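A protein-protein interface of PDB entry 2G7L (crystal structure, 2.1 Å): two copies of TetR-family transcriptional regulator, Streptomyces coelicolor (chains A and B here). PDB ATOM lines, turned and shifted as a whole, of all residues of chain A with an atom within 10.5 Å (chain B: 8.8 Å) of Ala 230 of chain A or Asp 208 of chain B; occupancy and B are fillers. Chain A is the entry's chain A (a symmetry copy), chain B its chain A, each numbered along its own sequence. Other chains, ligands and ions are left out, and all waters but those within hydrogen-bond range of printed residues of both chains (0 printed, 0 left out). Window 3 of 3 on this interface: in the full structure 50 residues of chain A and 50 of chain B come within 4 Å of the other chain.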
ATOM      1  N   ALA A 143       9.019   8.340 -12.845  1.00  0.00           N
ATOM      2  CA  ALA A 143       8.568   7.101 -13.485  1.00  0.00           C
ATOM      3  C   ALA A 143       7.092   6.852 -13.179  1.00  0.00           C
ATOM      4  O   ALA A 143       6.310   6.463 -14.055  1.00  0.00           O
ATOM      5  CB  ALA A 143       9.412   5.935 -13.067  1.00  0.00           C
ATOM      6  N   TRP A 147       4.075   6.646 -16.016  1.00  0.00           N
ATOM      7  CA  TRP A 147       3.176   5.497 -16.133  1.00  0.00           C
ATOM      8  C   TRP A 147       1.804   5.793 -15.546  1.00  0.00           C
ATOM      9  O   TRP A 147       0.776   5.276 -16.019  1.00  0.00           O
ATOM     10  CB  TRP A 147       3.826   4.256 -15.530  1.00  0.00           C
ATOM     11  CG  TRP A 147       5.005   3.737 -16.322  1.00  0.00           C
ATOM     12  CD1 TRP A 147       5.722   4.407 -17.239  1.00  0.00           C
ATOM     13  CD2 TRP A 147       5.592   2.421 -16.234  1.00  0.00           C
ATOM     14  NE1 TRP A 147       6.784   3.599 -17.727  1.00  0.00           N
ATOM     15  CE2 TRP A 147       6.702   2.383 -17.106  1.00  0.00           C
ATOM     16  CE3 TRP A 147       5.263   1.265 -15.517  1.00  0.00           C
ATOM     17  CZ2 TRP A 147       7.493   1.220 -17.284  1.00  0.00           C
ATOM     18  CZ3 TRP A 147       6.049   0.146 -15.672  1.00  0.00           C
ATOM     19  CH2 TRP A 147       7.148   0.127 -16.540  1.00  0.00           C
ATOM     20  N   LYS A 151      -2.292   5.376 -17.067  1.00  0.00           N
ATOM     21  CA  LYS A 151      -3.302   4.652 -16.288  1.00  0.00           C
ATOM     22  C   LYS A 151      -4.506   5.470 -15.973  1.00  0.00           C
ATOM     23  O   LYS A 151      -5.611   4.964 -16.068  1.00  0.00           O
ATOM     24  CB  LYS A 151      -2.699   4.097 -14.966  1.00  0.00           C
ATOM     25  CG  LYS A 151      -1.980   2.771 -15.237  1.00  0.00           C
ATOM     26  CD  LYS A 151      -0.449   2.820 -15.240  1.00  0.00           C
ATOM     27  CE  LYS A 151       0.287   1.835 -16.341  1.00  0.00           C
ATOM     28  NZ  LYS A 151       0.935   2.776 -17.405  1.00  0.00           N
ATOM     29  N   THR A 224       3.497   3.613  -5.387  1.00  0.00           N
ATOM     30  CA  THR A 224       4.050   2.369  -5.940  1.00  0.00           C
ATOM     31  C   THR A 224       5.184   2.644  -6.894  1.00  0.00           C
ATOM     32  O   THR A 224       4.963   3.172  -7.951  1.00  0.00           O
ATOM     33  CB  THR A 224       2.953   1.543  -6.715  1.00  0.00           C
ATOM     34  OG1 THR A 224       1.756   1.417  -5.937  1.00  0.00           O
ATOM     35  CG2 THR A 224       3.465   0.202  -7.079  1.00  0.00           C
ATOM     36  N   PRO A 225       6.416   2.296  -6.519  1.00  0.00           N
ATOM     37  CA  PRO A 225       7.581   2.411  -7.403  1.00  0.00           C
ATOM     38  C   PRO A 225       7.449   1.574  -8.686  1.00  0.00           C
ATOM     39  O   PRO A 225       6.879   0.452  -8.654  1.00  0.00           O
ATOM     40  CB  PRO A 225       8.719   1.841  -6.554  1.00  0.00           C
ATOM     41  CG  PRO A 225       8.271   2.033  -5.155  1.00  0.00           C
ATOM     42  CD  PRO A 225       6.793   1.806  -5.173  1.00  0.00           C
ATOM     43  N   VAL A 226       7.952   2.127  -9.798  1.00  0.00           N
ATOM     44  CA  VAL A 226       8.105   1.372 -11.007  1.00  0.00           C
ATOM     45  C   VAL A 226       9.403   0.591 -11.058  1.00  0.00           C
ATOM     46  O   VAL A 226      10.505   1.160 -10.929  1.00  0.00           O
ATOM     47  CB  VAL A 226       7.630   2.099 -12.354  1.00  0.00           C
ATOM     48  CG1 VAL A 226       6.922   3.334 -12.112  1.00  0.00           C
ATOM     49  CG2 VAL A 226       8.646   2.150 -13.392  1.00  0.00           C
ATOM     50  N   PRO A 227       9.269  -0.750 -11.130  1.00  0.00           N
ATOM     51  CA  PRO A 227      10.446  -1.598 -11.087  1.00  0.00           C
ATOM     52  C   PRO A 227      11.254  -1.419 -12.329  1.00  0.00           C
ATOM     53  O   PRO A 227      10.811  -0.742 -13.263  1.00  0.00           O
ATOM     54  CB  PRO A 227       9.853  -3.023 -10.993  1.00  0.00           C
ATOM     55  CG  PRO A 227       8.519  -2.810 -10.373  1.00  0.00           C
ATOM     56  CD  PRO A 227       8.042  -1.561 -11.169  1.00  0.00           C
ATOM     57  N   GLY A 228      12.461  -1.965 -12.340  1.00  0.00           N
ATOM     58  CA  GLY A 228      13.229  -2.002 -13.578  1.00  0.00           C
ATOM     59  C   GLY A 228      12.679  -3.090 -14.510  1.00  0.00           C
ATOM     60  O   GLY A 228      11.772  -3.839 -14.123  1.00  0.00           O
ATOM     61  N   PRO A 229      13.236  -3.194 -15.737  1.00  0.00           N
ATOM     62  CA  PRO A 229      13.007  -4.230 -16.754  1.00  0.00           C
ATOM     63  C   PRO A 229      12.735  -5.670 -16.248  1.00  0.00           C
ATOM     64  O   PRO A 229      13.501  -6.188 -15.404  1.00  0.00           O
ATOM     65  CB  PRO A 229      14.339  -4.235 -17.528  1.00  0.00           C
ATOM     66  CG  PRO A 229      15.187  -3.064 -16.966  1.00  0.00           C
ATOM     67  CD  PRO A 229      14.217  -2.204 -16.220  1.00  0.00           C
ATOM     68  N   ALA A 230      11.680  -6.309 -16.798  1.00  0.00           N
ATOM     69  CA  ALA A 230      11.314  -7.746 -16.540  1.00  0.00           C
ATOM     70  C   ALA A 230      12.501  -8.728 -16.481  1.00  0.00           C
ATOM     71  O   ALA A 230      12.376  -9.897 -16.882  1.00  0.00           O
ATOM     72  CB  ALA A 230      10.317  -8.240 -17.597  1.00  0.00           C
ATOM     73  N   ARG B  94      -2.573 -12.086  -8.122  1.00  0.00           N
ATOM     74  CA  ARG B  94      -1.854 -11.708  -9.306  1.00  0.00           C
ATOM     75  C   ARG B  94      -1.865 -12.846 -10.353  1.00  0.00           C
ATOM     76  O   ARG B  94      -1.993 -12.586 -11.583  1.00  0.00           O
ATOM     77  CB  ARG B  94      -0.414 -11.313  -8.959  1.00  0.00           C
ATOM     78  CG  ARG B  94       0.311 -10.659 -10.155  1.00  0.00           C
ATOM     79  CD  ARG B  94       1.846 -10.555 -10.002  1.00  0.00           C
ATOM     80  NE  ARG B  94       2.282  -9.619  -8.932  1.00  0.00           N
ATOM     81  CZ  ARG B  94       2.572  -8.323  -9.085  1.00  0.00           C
ATOM     82  NH1 ARG B  94       2.425  -7.716 -10.262  1.00  0.00           N
ATOM     83  NH2 ARG B  94       2.990  -7.614  -8.040  1.00  0.00           N
ATOM     84  N   PHE B 105      -5.431 -11.501 -24.141  1.00  0.00           N
ATOM     85  CA  PHE B 105      -4.375 -11.152 -25.110  1.00  0.00           C
ATOM     86  C   PHE B 105      -4.444 -12.069 -26.330  1.00  0.00           C
ATOM     87  O   PHE B 105      -4.117 -11.647 -27.423  1.00  0.00           O
ATOM     88  CB  PHE B 105      -2.971 -11.282 -24.483  1.00  0.00           C
ATOM     89  CG  PHE B 105      -2.453 -10.003 -23.769  1.00  0.00           C
ATOM     90  CD1 PHE B 105      -3.266  -9.280 -22.891  1.00  0.00           C
ATOM     91  CD2 PHE B 105      -1.145  -9.563 -23.971  1.00  0.00           C
ATOM     92  CE1 PHE B 105      -2.784  -8.088 -22.205  1.00  0.00           C
ATOM     93  CE2 PHE B 105      -0.649  -8.411 -23.280  1.00  0.00           C
ATOM     94  CZ  PHE B 105      -1.495  -7.669 -22.404  1.00  0.00           C
ATOM     95  N   THR B 159      -6.424  -3.148 -20.932  1.00  0.00           N
ATOM     96  CA  THR B 159      -5.049  -3.338 -21.461  1.00  0.00           C
ATOM     97  C   THR B 159      -4.960  -4.377 -22.590  1.00  0.00           C
ATOM     98  O   THR B 159      -4.152  -4.252 -23.528  1.00  0.00           O
ATOM     99  CB  THR B 159      -4.018  -3.699 -20.345  1.00  0.00           C
ATOM    100  OG1 THR B 159      -3.963  -2.650 -19.359  1.00  0.00           O
ATOM    101  CG2 THR B 159      -2.587  -3.849 -20.927  1.00  0.00           C
ATOM    102  N   ALA B 203       8.033   4.036 -22.366  1.00  0.00           N
ATOM    103  CA  ALA B 203       8.755   2.785 -22.085  1.00  0.00           C
ATOM    104  C   ALA B 203       7.991   1.654 -21.337  1.00  0.00           C
ATOM    105  O   ALA B 203       6.915   1.869 -20.706  1.00  0.00           O
ATOM    106  CB  ALA B 203      10.119   3.082 -21.423  1.00  0.00           C
ATOM    107  N   GLY B 204       8.560   0.454 -21.463  1.00  0.00           N
ATOM    108  CA  GLY B 204       8.078  -0.766 -20.813  1.00  0.00           C
ATOM    109  C   GLY B 204       7.221  -1.679 -21.671  1.00  0.00           C
ATOM    110  O   GLY B 204       6.420  -1.209 -22.498  1.00  0.00           O
ATOM    111  N   SER B 205       7.381  -2.985 -21.455  1.00  0.00           N
ATOM    112  CA  SER B 205       6.533  -4.035 -22.052  1.00  0.00           C
ATOM    113  C   SER B 205       5.118  -3.942 -21.512  1.00  0.00           C
ATOM    114  O   SER B 205       4.901  -3.356 -20.467  1.00  0.00           O
ATOM    115  CB  SER B 205       7.111  -5.409 -21.730  1.00  0.00           C
ATOM    116  OG  SER B 205       7.133  -5.721 -20.319  1.00  0.00           O
ATOM    117  N   ALA B 206       4.146  -4.508 -22.227  1.00  0.00           N
ATOM    118  CA  ALA B 206       2.757  -4.565 -21.718  1.00  0.00           C
ATOM    119  C   ALA B 206       2.688  -5.367 -20.415  1.00  0.00           C
ATOM    120  O   ALA B 206       1.808  -5.121 -19.572  1.00  0.00           O
ATOM    121  CB  ALA B 206       1.805  -5.161 -22.779  1.00  0.00           C
ATOM    122  N   HIS B 207       3.610  -6.332 -20.307  1.00  0.00           N
ATOM    123  CA  HIS B 207       3.894  -7.137 -19.103  1.00  0.00           C
ATOM    124  C   HIS B 207       4.411  -6.308 -17.919  1.00  0.00           C
ATOM    125  O   HIS B 207       3.975  -6.489 -16.754  1.00  0.00           O
ATOM    126  CB  HIS B 207       4.962  -8.217 -19.429  1.00  0.00           C
ATOM    127  CG  HIS B 207       5.611  -8.841 -18.210  1.00  0.00           C
ATOM    128  ND1 HIS B 207       4.999  -9.828 -17.450  1.00  0.00           N
ATOM    129  CD2 HIS B 207       6.820  -8.618 -17.629  1.00  0.00           C
ATOM    130  CE1 HIS B 207       5.805 -10.182 -16.459  1.00  0.00           C
ATOM    131  NE2 HIS B 207       6.913  -9.460 -16.539  1.00  0.00           N
ATOM    132  N   ASP B 208       5.367  -5.427 -18.226  1.00  0.00           N
ATOM    133  CA  ASP B 208       5.938  -4.501 -17.216  1.00  0.00           C
ATOM    134  C   ASP B 208       4.824  -3.584 -16.707  1.00  0.00           C
ATOM    135  O   ASP B 208       4.646  -3.457 -15.536  1.00  0.00           O
ATOM    136  CB  ASP B 208       7.080  -3.701 -17.811  1.00  0.00           C
ATOM    137  CG  ASP B 208       8.361  -4.521 -17.973  1.00  0.00           C
ATOM    138  OD1 ASP B 208       8.645  -5.459 -17.144  1.00  0.00           O
ATOM    139  OD2 ASP B 208       9.107  -4.188 -18.941  1.00  0.00           O
ATOM    140  N   ARG B 209       4.027  -3.031 -17.610  1.00  0.00           N
ATOM    141  CA  ARG B 209       2.988  -2.083 -17.254  1.00  0.00           C
ATOM    142  C   ARG B 209       1.905  -2.747 -16.444  1.00  0.00           C
ATOM    143  O   ARG B 209       1.330  -2.159 -15.562  1.00  0.00           O
ATOM    144  CB  ARG B 209       2.414  -1.452 -18.532  1.00  0.00           C
ATOM    145  CG  ARG B 209       3.470  -0.631 -19.390  1.00  0.00           C
ATOM    146  CD  ARG B 209       3.644   0.722 -18.788  1.00  0.00           C
ATOM    147  NE  ARG B 209       4.385   1.659 -19.625  1.00  0.00           N
ATOM    148  CZ  ARG B 209       3.958   2.875 -19.910  1.00  0.00           C
ATOM    149  NH1 ARG B 209       4.691   3.630 -20.713  1.00  0.00           N
ATOM    150  NH2 ARG B 209       2.789   3.330 -19.405  1.00  0.00           N
ATOM    151  N   LEU B 210       1.600  -3.998 -16.777  1.00  0.00           N
ATOM    152  CA  LEU B 210       0.587  -4.781 -16.075  1.00  0.00           C
ATOM    153  C   LEU B 210       1.111  -5.247 -14.728  1.00  0.00           C
ATOM    154  O   LEU B 210       0.342  -5.348 -13.798  1.00  0.00           O
ATOM    155  CB  LEU B 210       0.195  -6.029 -16.939  1.00  0.00           C
ATOM    156  CG  LEU B 210      -0.894  -5.948 -18.034  1.00  0.00           C
ATOM    157  CD1 LEU B 210      -0.838  -7.219 -18.847  1.00  0.00           C
ATOM    158  CD2 LEU B 210      -2.343  -5.713 -17.436  1.00  0.00           C
ATOM    159  N   ARG B 211       2.399  -5.545 -14.602  1.00  0.00           N
ATOM    160  CA  ARG B 211       2.958  -5.876 -13.232  1.00  0.00           C
ATOM    161  C   ARG B 211       2.775  -4.673 -12.330  1.00  0.00           C
ATOM    162  O   ARG B 211       2.276  -4.757 -11.211  1.00  0.00           O
ATOM    163  CB  ARG B 211       4.462  -6.247 -13.250  1.00  0.00           C
ATOM    164  CG  ARG B 211       4.820  -7.746 -13.466  1.00  0.00           C
ATOM    165  CD  ARG B 211       6.263  -8.099 -13.034  1.00  0.00           C
ATOM    166  NE  ARG B 211       6.471  -7.986 -11.575  1.00  0.00           N
ATOM    167  CZ  ARG B 211       6.128  -8.930 -10.679  1.00  0.00           C
ATOM    168  NH1 ARG B 211       5.551 -10.079 -11.072  1.00  0.00           N
ATOM    169  NH2 ARG B 211       6.349  -8.729  -9.381  1.00  0.00           N
ATOM    170  N   TRP B 212       3.145  -3.518 -12.869  1.00  0.00           N
ATOM    171  CA  TRP B 212       2.956  -2.252 -12.145  1.00  0.00           C
ATOM    172  C   TRP B 212       1.488  -1.897 -11.884  1.00  0.00           C
ATOM    173  O   TRP B 212       1.157  -1.556 -10.776  1.00  0.00           O
ATOM    174  CB  TRP B 212       3.674  -1.087 -12.899  1.00  0.00           C
ATOM    175  CG  TRP B 212       3.712   0.164 -12.095  1.00  0.00           C
ATOM    176  CD1 TRP B 212       4.435   0.375 -10.956  1.00  0.00           C
ATOM    177  CD2 TRP B 212       2.965   1.379 -12.330  1.00  0.00           C
ATOM    178  NE1 TRP B 212       4.196   1.622 -10.470  1.00  0.00           N
ATOM    179  CE2 TRP B 212       3.317   2.279 -11.289  1.00  0.00           C
ATOM    180  CE3 TRP B 212       2.038   1.791 -13.319  1.00  0.00           C
ATOM    181  CZ2 TRP B 212       2.785   3.567 -11.190  1.00  0.00           C
ATOM    182  CZ3 TRP B 212       1.471   3.048 -13.202  1.00  0.00           C
ATOM    183  CH2 TRP B 212       1.879   3.947 -12.159  1.00  0.00           C
ATOM    184  N   SER B 213       0.566  -1.927 -12.859  1.00  0.00           N
ATOM    185  CA  SER B 213      -0.765  -1.446 -12.415  1.00  0.00           C
ATOM    186  C   SER B 213      -1.521  -2.384 -11.449  1.00  0.00           C
ATOM    187  O   SER B 213      -2.427  -1.970 -10.656  1.00  0.00           O
ATOM    188  CB  SER B 213      -1.638  -1.057 -13.592  1.00  0.00           C
ATOM    189  OG  SER B 213      -1.950  -2.179 -14.329  1.00  0.00           O
ATOM    190  N   PHE B 214      -1.186  -3.656 -11.497  1.00  0.00           N
ATOM    191  CA  PHE B 214      -1.706  -4.573 -10.470  1.00  0.00           C
ATOM    192  C   PHE B 214      -1.385  -4.064  -9.045  1.00  0.00           C
ATOM    193  O   PHE B 214      -2.277  -3.846  -8.184  1.00  0.00           O
ATOM    194  CB  PHE B 214      -1.147  -6.005 -10.688  1.00  0.00           C
ATOM    195  CG  PHE B 214      -1.500  -6.949  -9.553  1.00  0.00           C
ATOM    196  CD1 PHE B 214      -2.724  -7.606  -9.535  1.00  0.00           C
ATOM    197  CD2 PHE B 214      -0.653  -7.107  -8.460  1.00  0.00           C
ATOM    198  CE1 PHE B 214      -3.066  -8.445  -8.427  1.00  0.00           C
ATOM    199  CE2 PHE B 214      -1.002  -7.943  -7.359  1.00  0.00           C
ATOM    200  CZ  PHE B 214      -2.193  -8.611  -7.367  1.00  0.00           C
ATOM    201  N   ASP B 215      -0.099  -3.835  -8.804  1.00  0.00           N
ATOM    202  CA  ASP B 215       0.347  -3.192  -7.509  1.00  0.00           C
ATOM    203  C   ASP B 215      -0.258  -1.835  -7.268  1.00  0.00           C
ATOM    204  O   ASP B 215      -0.763  -1.570  -6.197  1.00  0.00           O
ATOM    205  CB  ASP B 215       1.881  -3.108  -7.502  1.00  0.00           C
ATOM    206  CG  ASP B 215       2.513  -4.473  -7.353  1.00  0.00           C
ATOM    207  OD1 ASP B 215       1.944  -5.228  -6.536  1.00  0.00           O
ATOM    208  OD2 ASP B 215       3.553  -4.779  -8.010  1.00  0.00           O
ATOM    209  N   VAL B 216      -0.306  -0.992  -8.292  1.00  0.00           N
ATOM    210  CA  VAL B 216      -0.926   0.321  -8.117  1.00  0.00           C
ATOM    211  C   VAL B 216      -2.347   0.154  -7.654  1.00  0.00           C
ATOM    212  O   VAL B 216      -2.843   0.850  -6.736  1.00  0.00           O
ATOM    213  CB  VAL B 216      -0.908   1.137  -9.505  1.00  0.00           C
ATOM    214  CG1 VAL B 216      -1.731   2.348  -9.438  1.00  0.00           C
ATOM    215  CG2 VAL B 216       0.468   1.419  -9.907  1.00  0.00           C
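The indole nitrogen (NE1) of Trp 212 of chain B sits at hydrogen-bond distance from the backbone carbonyl oxygen (O) of Thr 224 of chain A, 3.1 Å away.
The guanidinium group (NH2) of Arg 209 of chain B lies close to the side-chain amino group (NZ) of Lys 151 of chain A (2.8 Å).
The side-chain carboxylate (OD1) of Asp 208 of chain B sits at hydrogen-bond distance from the backbone NH (N) of Ala 230 of chain A (3.2 Å).
NE1 of Trp 212 of chain B sits close to O of Pro 225 of chain A (3.4 Å).
The backbone carbonyl oxygen of Ala 203 of chain B lies within hydrogen-bond range of the indole nitrogen of Trp 147 of chain A (3.4 Å).
The backbone carbonyl oxygen (O) of Ala 203 of chain B is in hydrogen-bond range of the guanidinium group (NE) of Arg 209 of chain B (2.8 Å).
The side-chain hydroxyl (OG) of Ser 205 of chain B sits at hydrogen-bond distance from the backbone NH (N) of Asp 208 of chain B, at 2.8 Å.
O of Trp 147 of chain A lies close to NZ of Lys 151 of chain A, at 2.9 Å.
NH2 of Arg 94 of chain B lies within salt-bridge range of OD2 of Asp 215 of chain B, 2.9 Å away.
Among the printed residues, merely in contact across the chains: Lys 151 of chain A with Trp 212 of chain B, Trp 147 of chain A with Arg 209 of chain B, Ala 230 of chain A with His 207 of chain B, Trp 147 of chain A with Trp 212 of chain B, Val 226 of chain A with Trp 212 of chain B, Thr 224 of chain A with Val 216 of chain B, Thr 224 of chain A with Asp 215 of chain B and Trp 147 of chain A with Asp 208 of chain B.
Of the printed residues of chain B, Trp 147 of chain A touches Ala 203, Asp 208, Arg 209 and Trp 212.
Ala 230 of chain A touches just these residues of chain B: His 207 and Asp 208.
Thr 159 of chain B touches none of the printed residues of chain A.
No residue of chain A comes within 4 Å of Gly 204 of chain B.
No residue of chain A comes within 4 Å of Ser 205 of chain B.
No residue of chain A comes within 4 Å of Ala 206 of chain B.
Printed residues of chain A within 4 Å of His 207 of chain B: Ala 230 (3.5 Å).
Asp 208 of chain B touches two residues of chain A.
Of the printed residues of chain A, Arg 209 of chain B touches Trp 147 (3.5 Å) and Lys 151 (2.8 Å).
Printed residues of chain A within 4 Å of Asp 215 of chain B: Thr 224 (3.7 Å).
Of the 10 printed residues of chain A, 6 touch a printed residue of chain B.
Hydrophobic or aromatic side chains of chain B within 4 Å of the printed part of chain A: His 207 and Trp 212.
No position is printed for both chains.
Of the 13 pairs that touch across the chains among the printed residues, none has its exchanged pair printed and touching as well.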
